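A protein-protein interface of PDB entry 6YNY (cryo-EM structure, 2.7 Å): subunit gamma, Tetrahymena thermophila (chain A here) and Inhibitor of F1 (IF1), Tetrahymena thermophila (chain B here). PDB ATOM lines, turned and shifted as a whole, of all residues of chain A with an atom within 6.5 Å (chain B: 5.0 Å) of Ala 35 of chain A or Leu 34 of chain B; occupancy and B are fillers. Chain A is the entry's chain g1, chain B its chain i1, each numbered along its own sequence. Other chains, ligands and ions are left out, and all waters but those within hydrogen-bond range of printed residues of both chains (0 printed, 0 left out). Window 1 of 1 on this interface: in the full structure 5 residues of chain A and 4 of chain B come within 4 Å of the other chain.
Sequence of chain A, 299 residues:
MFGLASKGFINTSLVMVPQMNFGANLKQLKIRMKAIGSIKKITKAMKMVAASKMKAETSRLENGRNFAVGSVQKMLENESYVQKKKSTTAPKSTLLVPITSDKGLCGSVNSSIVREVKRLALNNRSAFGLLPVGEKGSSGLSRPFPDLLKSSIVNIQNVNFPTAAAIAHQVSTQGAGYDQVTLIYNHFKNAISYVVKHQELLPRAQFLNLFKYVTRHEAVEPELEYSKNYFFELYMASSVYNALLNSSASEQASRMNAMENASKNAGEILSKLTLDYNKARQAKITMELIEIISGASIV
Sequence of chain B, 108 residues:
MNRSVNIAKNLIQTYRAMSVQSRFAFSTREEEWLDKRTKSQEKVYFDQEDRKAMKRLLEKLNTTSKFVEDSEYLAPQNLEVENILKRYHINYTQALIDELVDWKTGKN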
ATOM      1  N   LYS A  30      26.528  16.929   8.319  1.00  0.00           N
ATOM      2  CA  LYS A  30      25.823  16.604   9.555  1.00  0.00           C
ATOM      3  C   LYS A  30      24.519  17.381   9.672  1.00  0.00           C
ATOM      4  O   LYS A  30      23.570  16.910  10.309  1.00  0.00           O
ATOM      5  CB  LYS A  30      26.723  16.884  10.759  1.00  0.00           C
ATOM      6  CG  LYS A  30      26.083  16.562  12.100  1.00  0.00           C
ATOM      7  CD  LYS A  30      27.127  16.377  13.194  1.00  0.00           C
ATOM      8  CE  LYS A  30      27.961  17.632  13.402  1.00  0.00           C
ATOM      9  NZ  LYS A  30      28.966  17.457  14.486  1.00  0.00           N
ATOM     10  N   ILE A  31      24.450  18.565   9.064  1.00  0.00           N
ATOM     11  CA  ILE A  31      23.209  19.335   9.070  1.00  0.00           C
ATOM     12  C   ILE A  31      22.177  18.678   8.161  1.00  0.00           C
ATOM     13  O   ILE A  31      21.013  18.506   8.540  1.00  0.00           O
ATOM     14  CB  ILE A  31      23.481  20.792   8.659  1.00  0.00           C
ATOM     15  CG1 ILE A  31      24.252  21.514   9.767  1.00  0.00           C
ATOM     16  CG2 ILE A  31      22.172  21.510   8.351  1.00  0.00           C
ATOM     17  CD1 ILE A  31      24.813  22.859   9.355  1.00  0.00           C
ATOM     18  N   ARG A  32      22.588  18.304   6.948  1.00  0.00           N
ATOM     19  CA  ARG A  32      21.660  17.658   6.027  1.00  0.00           C
ATOM     20  C   ARG A  32      21.200  16.308   6.560  1.00  0.00           C
ATOM     21  O   ARG A  32      20.051  15.910   6.337  1.00  0.00           O
ATOM     22  CB  ARG A  32      22.309  17.500   4.653  1.00  0.00           C
ATOM     23  CG  ARG A  32      21.353  17.024   3.572  1.00  0.00           C
ATOM     24  CD  ARG A  32      21.838  17.415   2.185  1.00  0.00           C
ATOM     25  NE  ARG A  32      23.068  16.721   1.808  1.00  0.00           N
ATOM     26  CZ  ARG A  32      23.113  15.550   1.179  1.00  0.00           C
ATOM     27  NH1 ARG A  32      21.997  14.917   0.845  1.00  0.00           N
ATOM     28  NH2 ARG A  32      24.285  15.008   0.879  1.00  0.00           N
ATOM     29  N   MET A  33      22.079  15.590   7.264  1.00  0.00           N
ATOM     30  CA  MET A  33      21.666  14.350   7.911  1.00  0.00           C
ATOM     31  C   MET A  33      20.607  14.618   8.971  1.00  0.00           C
ATOM     32  O   MET A  33      19.666  13.831   9.136  1.00  0.00           O
ATOM     33  CB  MET A  33      22.878  13.652   8.526  1.00  0.00           C
ATOM     34  CG  MET A  33      23.845  13.077   7.504  1.00  0.00           C
ATOM     35  SD  MET A  33      25.357  12.436   8.251  1.00  0.00           S
ATOM     36  CE  MET A  33      24.691  11.199   9.362  1.00  0.00           C
ATOM     37  N   LYS A  34      20.744  15.726   9.703  1.00  0.00           N
ATOM     38  CA  LYS A  34      19.741  16.083  10.701  1.00  0.00           C
ATOM     39  C   LYS A  34      18.392  16.355  10.049  1.00  0.00           C
ATOM     40  O   LYS A  34      17.346  15.965  10.581  1.00  0.00           O
ATOM     41  CB  LYS A  34      20.209  17.304  11.492  1.00  0.00           C
ATOM     42  CG  LYS A  34      19.235  17.770  12.561  1.00  0.00           C
ATOM     43  CD  LYS A  34      19.769  18.982  13.306  1.00  0.00           C
ATOM     44  CE  LYS A  34      18.771  19.486  14.335  1.00  0.00           C
ATOM     45  NZ  LYS A  34      19.268  20.693  15.050  1.00  0.00           N
ATOM     46  N   ALA A  35      18.394  17.028   8.897  1.00  0.00           N
ATOM     47  CA  ALA A  35      17.141  17.330   8.212  1.00  0.00           C
ATOM     48  C   ALA A  35      16.422  16.052   7.800  1.00  0.00           C
ATOM     49  O   ALA A  35      15.213  15.906   8.019  1.00  0.00           O
ATOM     50  CB  ALA A  35      17.411  18.214   6.995  1.00  0.00           C
ATOM     51  N   ILE A  36      17.152  15.109   7.200  1.00  0.00           N
ATOM     52  CA  ILE A  36      16.537  13.850   6.787  1.00  0.00           C
ATOM     53  C   ILE A  36      16.021  13.089   8.000  1.00  0.00           C
ATOM     54  O   ILE A  36      14.985  12.415   7.933  1.00  0.00           O
ATOM     55  CB  ILE A  36      17.537  13.006   5.975  1.00  0.00           C
ATOM     56  CG1 ILE A  36      17.975  13.769   4.722  1.00  0.00           C
ATOM     57  CG2 ILE A  36      16.919  11.663   5.601  1.00  0.00           C
ATOM     58  CD1 ILE A  36      19.011  13.047   3.891  1.00  0.00           C
ATOM     59  N   GLY A  37      16.730  13.179   9.125  1.00  0.00           N
ATOM     60  CA  GLY A  37      16.259  12.519  10.330  1.00  0.00           C
ATOM     61  C   GLY A  37      14.921  13.056  10.798  1.00  0.00           C
ATOM     62  O   GLY A  37      14.034  12.293  11.186  1.00  0.00           O
ATOM     63  N   SER A  38      14.756  14.381  10.768  1.00  0.00           N
ATOM     64  CA  SER A  38      13.477  14.971  11.142  1.00  0.00           C
ATOM     65  C   SER A  38      12.387  14.593  10.148  1.00  0.00           C
ATOM     66  O   SER A  38      11.262  14.264  10.545  1.00  0.00           O
ATOM     67  CB  SER A  38      13.610  16.490  11.241  1.00  0.00           C
ATOM     68  OG  SER A  38      14.048  17.043  10.012  1.00  0.00           O
ATOM     69  N   ILE A  39      12.699  14.632   8.851  1.00  0.00           N
ATOM     70  CA  ILE A  39      11.721  14.249   7.837  1.00  0.00           C
ATOM     71  C   ILE A  39      11.257  12.817   8.065  1.00  0.00           C
ATOM     72  O   ILE A  39      10.054  12.530   8.090  1.00  0.00           O
ATOM     73  CB  ILE A  39      12.313  14.430   6.427  1.00  0.00           C
ATOM     74  CG1 ILE A  39      12.497  15.919   6.121  1.00  0.00           C
ATOM     75  CG2 ILE A  39      11.424  13.757   5.384  1.00  0.00           C
ATOM     76  CD1 ILE A  39      13.226  16.199   4.823  1.00  0.00           C
ATOM     77  N   LYS A  40      12.206  11.896   8.239  1.00  0.00           N
ATOM     78  CA  LYS A  40      11.844  10.509   8.513  1.00  0.00           C
ATOM     79  C   LYS A  40      11.035  10.399   9.798  1.00  0.00           C
ATOM     80  O   LYS A  40      10.110   9.584   9.891  1.00  0.00           O
ATOM     81  CB  LYS A  40      13.104   9.648   8.588  1.00  0.00           C
ATOM     82  CG  LYS A  40      12.841   8.180   8.874  1.00  0.00           C
ATOM     83  CD  LYS A  40      14.138   7.393   8.931  1.00  0.00           C
ATOM     84  CE  LYS A  40      13.893   5.947   9.320  1.00  0.00           C
ATOM     85  NZ  LYS A  40      15.165   5.181   9.436  1.00  0.00           N
ATOM     86  N   GLU B  30      18.514  20.087   1.713  1.00  0.00           N
ATOM     87  CA  GLU B  30      17.165  19.863   2.214  1.00  0.00           C
ATOM     88  C   GLU B  30      16.844  20.720   3.428  1.00  0.00           C
ATOM     89  O   GLU B  30      15.672  21.033   3.664  1.00  0.00           O
ATOM     90  CB  GLU B  30      16.974  18.387   2.568  1.00  0.00           C
ATOM     91  CG  GLU B  30      17.190  17.445   1.397  1.00  0.00           C
ATOM     92  CD  GLU B  30      16.903  16.000   1.752  1.00  0.00           C
ATOM     93  OE1 GLU B  30      16.330  15.755   2.833  1.00  0.00           O
ATOM     94  OE2 GLU B  30      17.250  15.109   0.949  1.00  0.00           O
ATOM     95  N   GLU B  31      17.858  21.105   4.206  1.00  0.00           N
ATOM     96  CA  GLU B  31      17.616  21.978   5.350  1.00  0.00           C
ATOM     97  C   GLU B  31      17.034  23.311   4.903  1.00  0.00           C
ATOM     98  O   GLU B  31      16.131  23.854   5.552  1.00  0.00           O
ATOM     99  CB  GLU B  31      18.914  22.193   6.127  1.00  0.00           C
ATOM    100  CG  GLU B  31      18.777  23.107   7.338  1.00  0.00           C
ATOM    101  CD  GLU B  31      17.803  22.571   8.371  1.00  0.00           C
ATOM    102  OE1 GLU B  31      17.441  21.378   8.289  1.00  0.00           O
ATOM    103  OE2 GLU B  31      17.397  23.345   9.263  1.00  0.00           O
ATOM    104  N   GLU B  32      17.539  23.859   3.796  1.00  0.00           N
ATOM    105  CA  GLU B  32      16.993  25.109   3.282  1.00  0.00           C
ATOM    106  C   GLU B  32      15.551  24.929   2.828  1.00  0.00           C
ATOM    107  O   GLU B  32      14.716  25.819   3.022  1.00  0.00           O
ATOM    108  CB  GLU B  32      17.857  25.622   2.129  1.00  0.00           C
ATOM    109  CG  GLU B  32      19.327  25.795   2.479  1.00  0.00           C
ATOM    110  CD  GLU B  32      19.558  26.862   3.532  1.00  0.00           C
ATOM    111  OE1 GLU B  32      18.606  27.608   3.845  1.00  0.00           O
ATOM    112  OE2 GLU B  32      20.692  26.955   4.047  1.00  0.00           O
ATOM    113  N   TRP B  33      15.239  23.778   2.229  1.00  0.00           N
ATOM    114  CA  TRP B  33      13.873  23.519   1.787  1.00  0.00           C
ATOM    115  C   TRP B  33      12.906  23.535   2.964  1.00  0.00           C
ATOM    116  O   TRP B  33      11.849  24.174   2.908  1.00  0.00           O
ATOM    117  CB  TRP B  33      13.818  22.178   1.055  1.00  0.00           C
ATOM    118  CG  TRP B  33      12.452  21.795   0.588  1.00  0.00           C
ATOM    119  CD1 TRP B  33      11.809  22.248  -0.526  1.00  0.00           C
ATOM    120  CD2 TRP B  33      11.561  20.867   1.216  1.00  0.00           C
ATOM    121  NE1 TRP B  33      10.570  21.663  -0.628  1.00  0.00           N
ATOM    122  CE2 TRP B  33      10.395  20.810   0.430  1.00  0.00           C
ATOM    123  CE3 TRP B  33      11.636  20.079   2.369  1.00  0.00           C
ATOM    124  CZ2 TRP B  33       9.312  19.997   0.758  1.00  0.00           C
ATOM    125  CZ3 TRP B  33      10.561  19.273   2.693  1.00  0.00           C
ATOM    126  CH2 TRP B  33       9.415  19.239   1.892  1.00  0.00           C
ATOM    127  N   LEU B  34      13.254  22.832   4.043  1.00  0.00           N
ATOM    128  CA  LEU B  34      12.413  22.849   5.236  1.00  0.00           C
ATOM    129  C   LEU B  34      12.340  24.245   5.838  1.00  0.00           C
ATOM    130  O   LEU B  34      11.273  24.684   6.283  1.00  0.00           O
ATOM    131  CB  LEU B  34      12.948  21.853   6.265  1.00  0.00           C
ATOM    132  CG  LEU B  34      12.919  20.380   5.852  1.00  0.00           C
ATOM    133  CD1 LEU B  34      13.742  19.545   6.818  1.00  0.00           C
ATOM    134  CD2 LEU B  34      11.490  19.866   5.787  1.00  0.00           C
ATOM    135  N   ASP B  35      13.468  24.958   5.864  1.00  0.00           N
ATOM    136  CA  ASP B  35      13.486  26.298   6.441  1.00  0.00           C
ATOM    137  C   ASP B  35      12.566  27.237   5.671  1.00  0.00           C
ATOM    138  O   ASP B  35      11.777  27.980   6.267  1.00  0.00           O
ATOM    139  CB  ASP B  35      14.916  26.837   6.458  1.00  0.00           C
ATOM    140  CG  ASP B  35      15.011  28.214   7.080  1.00  0.00           C
ATOM    141  OD1 ASP B  35      14.836  28.326   8.311  1.00  0.00           O
ATOM    142  OD2 ASP B  35      15.259  29.187   6.337  1.00  0.00           O
ATOM    143  N   LYS B  36      12.655  27.218   4.341  1.00  0.00           N
ATOM    144  CA  LYS B  36      11.790  28.072   3.534  1.00  0.00           C
ATOM    145  C   LYS B  36      10.327  27.693   3.710  1.00  0.00           C
ATOM    146  O   LYS B  36       9.462  28.567   3.844  1.00  0.00           O
ATOM    147  CB  LYS B  36      12.194  27.983   2.063  1.00  0.00           C
ATOM    148  CG  LYS B  36      13.598  28.484   1.774  1.00  0.00           C
ATOM    149  CD  LYS B  36      13.999  28.203   0.334  1.00  0.00           C
ATOM    150  CE  LYS B  36      15.416  28.670   0.047  1.00  0.00           C
ATOM    151  NZ  LYS B  36      15.574  30.137   0.239  1.00  0.00           N
ATOM    152  N   ARG B  37      10.029  26.392   3.711  1.00  0.00           N
ATOM    153  CA  ARG B  37       8.653  25.951   3.913  1.00  0.00           C
ATOM    154  C   ARG B  37       8.112  26.440   5.250  1.00  0.00           C
ATOM    155  O   ARG B  37       6.945  26.841   5.347  1.00  0.00           O
ATOM    156  CB  ARG B  37       8.574  24.426   3.827  1.00  0.00           C
ATOM    157  CG  ARG B  37       8.716  23.875   2.415  1.00  0.00           C
ATOM    158  CD  ARG B  37       7.467  24.128   1.584  1.00  0.00           C
ATOM    159  NE  ARG B  37       6.311  23.393   2.091  1.00  0.00           N
ATOM    160  CZ  ARG B  37       5.944  22.181   1.681  1.00  0.00           C
ATOM    161  NH1 ARG B  37       6.637  21.543   0.747  1.00  0.00           N
ATOM    162  NH2 ARG B  37       4.875  21.602   2.209  1.00  0.00           N
ATOM    163  N   THR B  38       8.943  26.416   6.292  1.00  0.00           N
ATOM    164  CA  THR B  38       8.512  26.897   7.599  1.00  0.00           C
ATOM    165  C   THR B  38       8.143  28.374   7.541  1.00  0.00           C
ATOM    166  O   THR B  38       7.020  28.765   7.880  1.00  0.00           O
ATOM    167  CB  THR B  38       9.617  26.661   8.631  1.00  0.00           C
ATOM    168  OG1 THR B  38       9.904  25.259   8.719  1.00  0.00           O
ATOM    169  CG2 THR B  38       9.195  27.179   9.999  1.00  0.00           C
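Ala 35 of chain A touches two residues of chain B. Of chain A, only Ala 35 (3.9 Å) and Ile 39 (3.9 Å) come within 4 Å of Leu 34 of chain B. Printed residues of chain B within 4 Å of Ile 31 of chain A: Glu 31. Of the printed residues of chain A, Glu 31 of chain B touches Ile 31 and Ala 35. Printed residues of chain B within 4 Å of Ile 36 of chain A: Glu 30 (3.2 Å). Printed residues of chain A within 4 Å of Glu 30 of chain B: Ile 36 (3.2 Å) and Ile 39 (3.7 Å). Lys 30 of chain A touches none of the printed residues of chain B. Ser 38 of chain A touches none of the printed residues of chain B.
Of the 9 printed residues of chain B, 3 touch a printed residue of chain A. Hydrophobic or aromatic side chains of chain B within 4 Å of the printed part of chain A: Leu 34. Printed residues of chain A that touch a printed residue of chain B: Ile 31, Ala 35, Ile 36 and Ile 39. Among the printed residues, no Asp or Glu carboxylate lies within 4 Å of a Lys or Arg side-chain nitrogen of the other chain.
Among the printed residues, pairs that only touch across the chains: Ile 31 of chain A with Glu 31 of chain B, Ala 35 of chain A with Glu 31 of chain B, Ala 35 of chain A with Leu 34 of chain B, Ile 36 of chain A with Glu 30 of chain B, Ile 39 of chain A with Glu 30 of chain B and Ile 39 of chain A with Leu 34 of chain B.
The backbone carbonyl oxygen (O) of Leu 34 of chain B lies within hydrogen-bond range of the side-chain hydroxyl (OG1) of Thr 38 of chain B (2.9 Å). OG of Ser 38 of chain A sits at hydrogen-bond distance from O of Ala 35 of chain A (2.6 Å).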
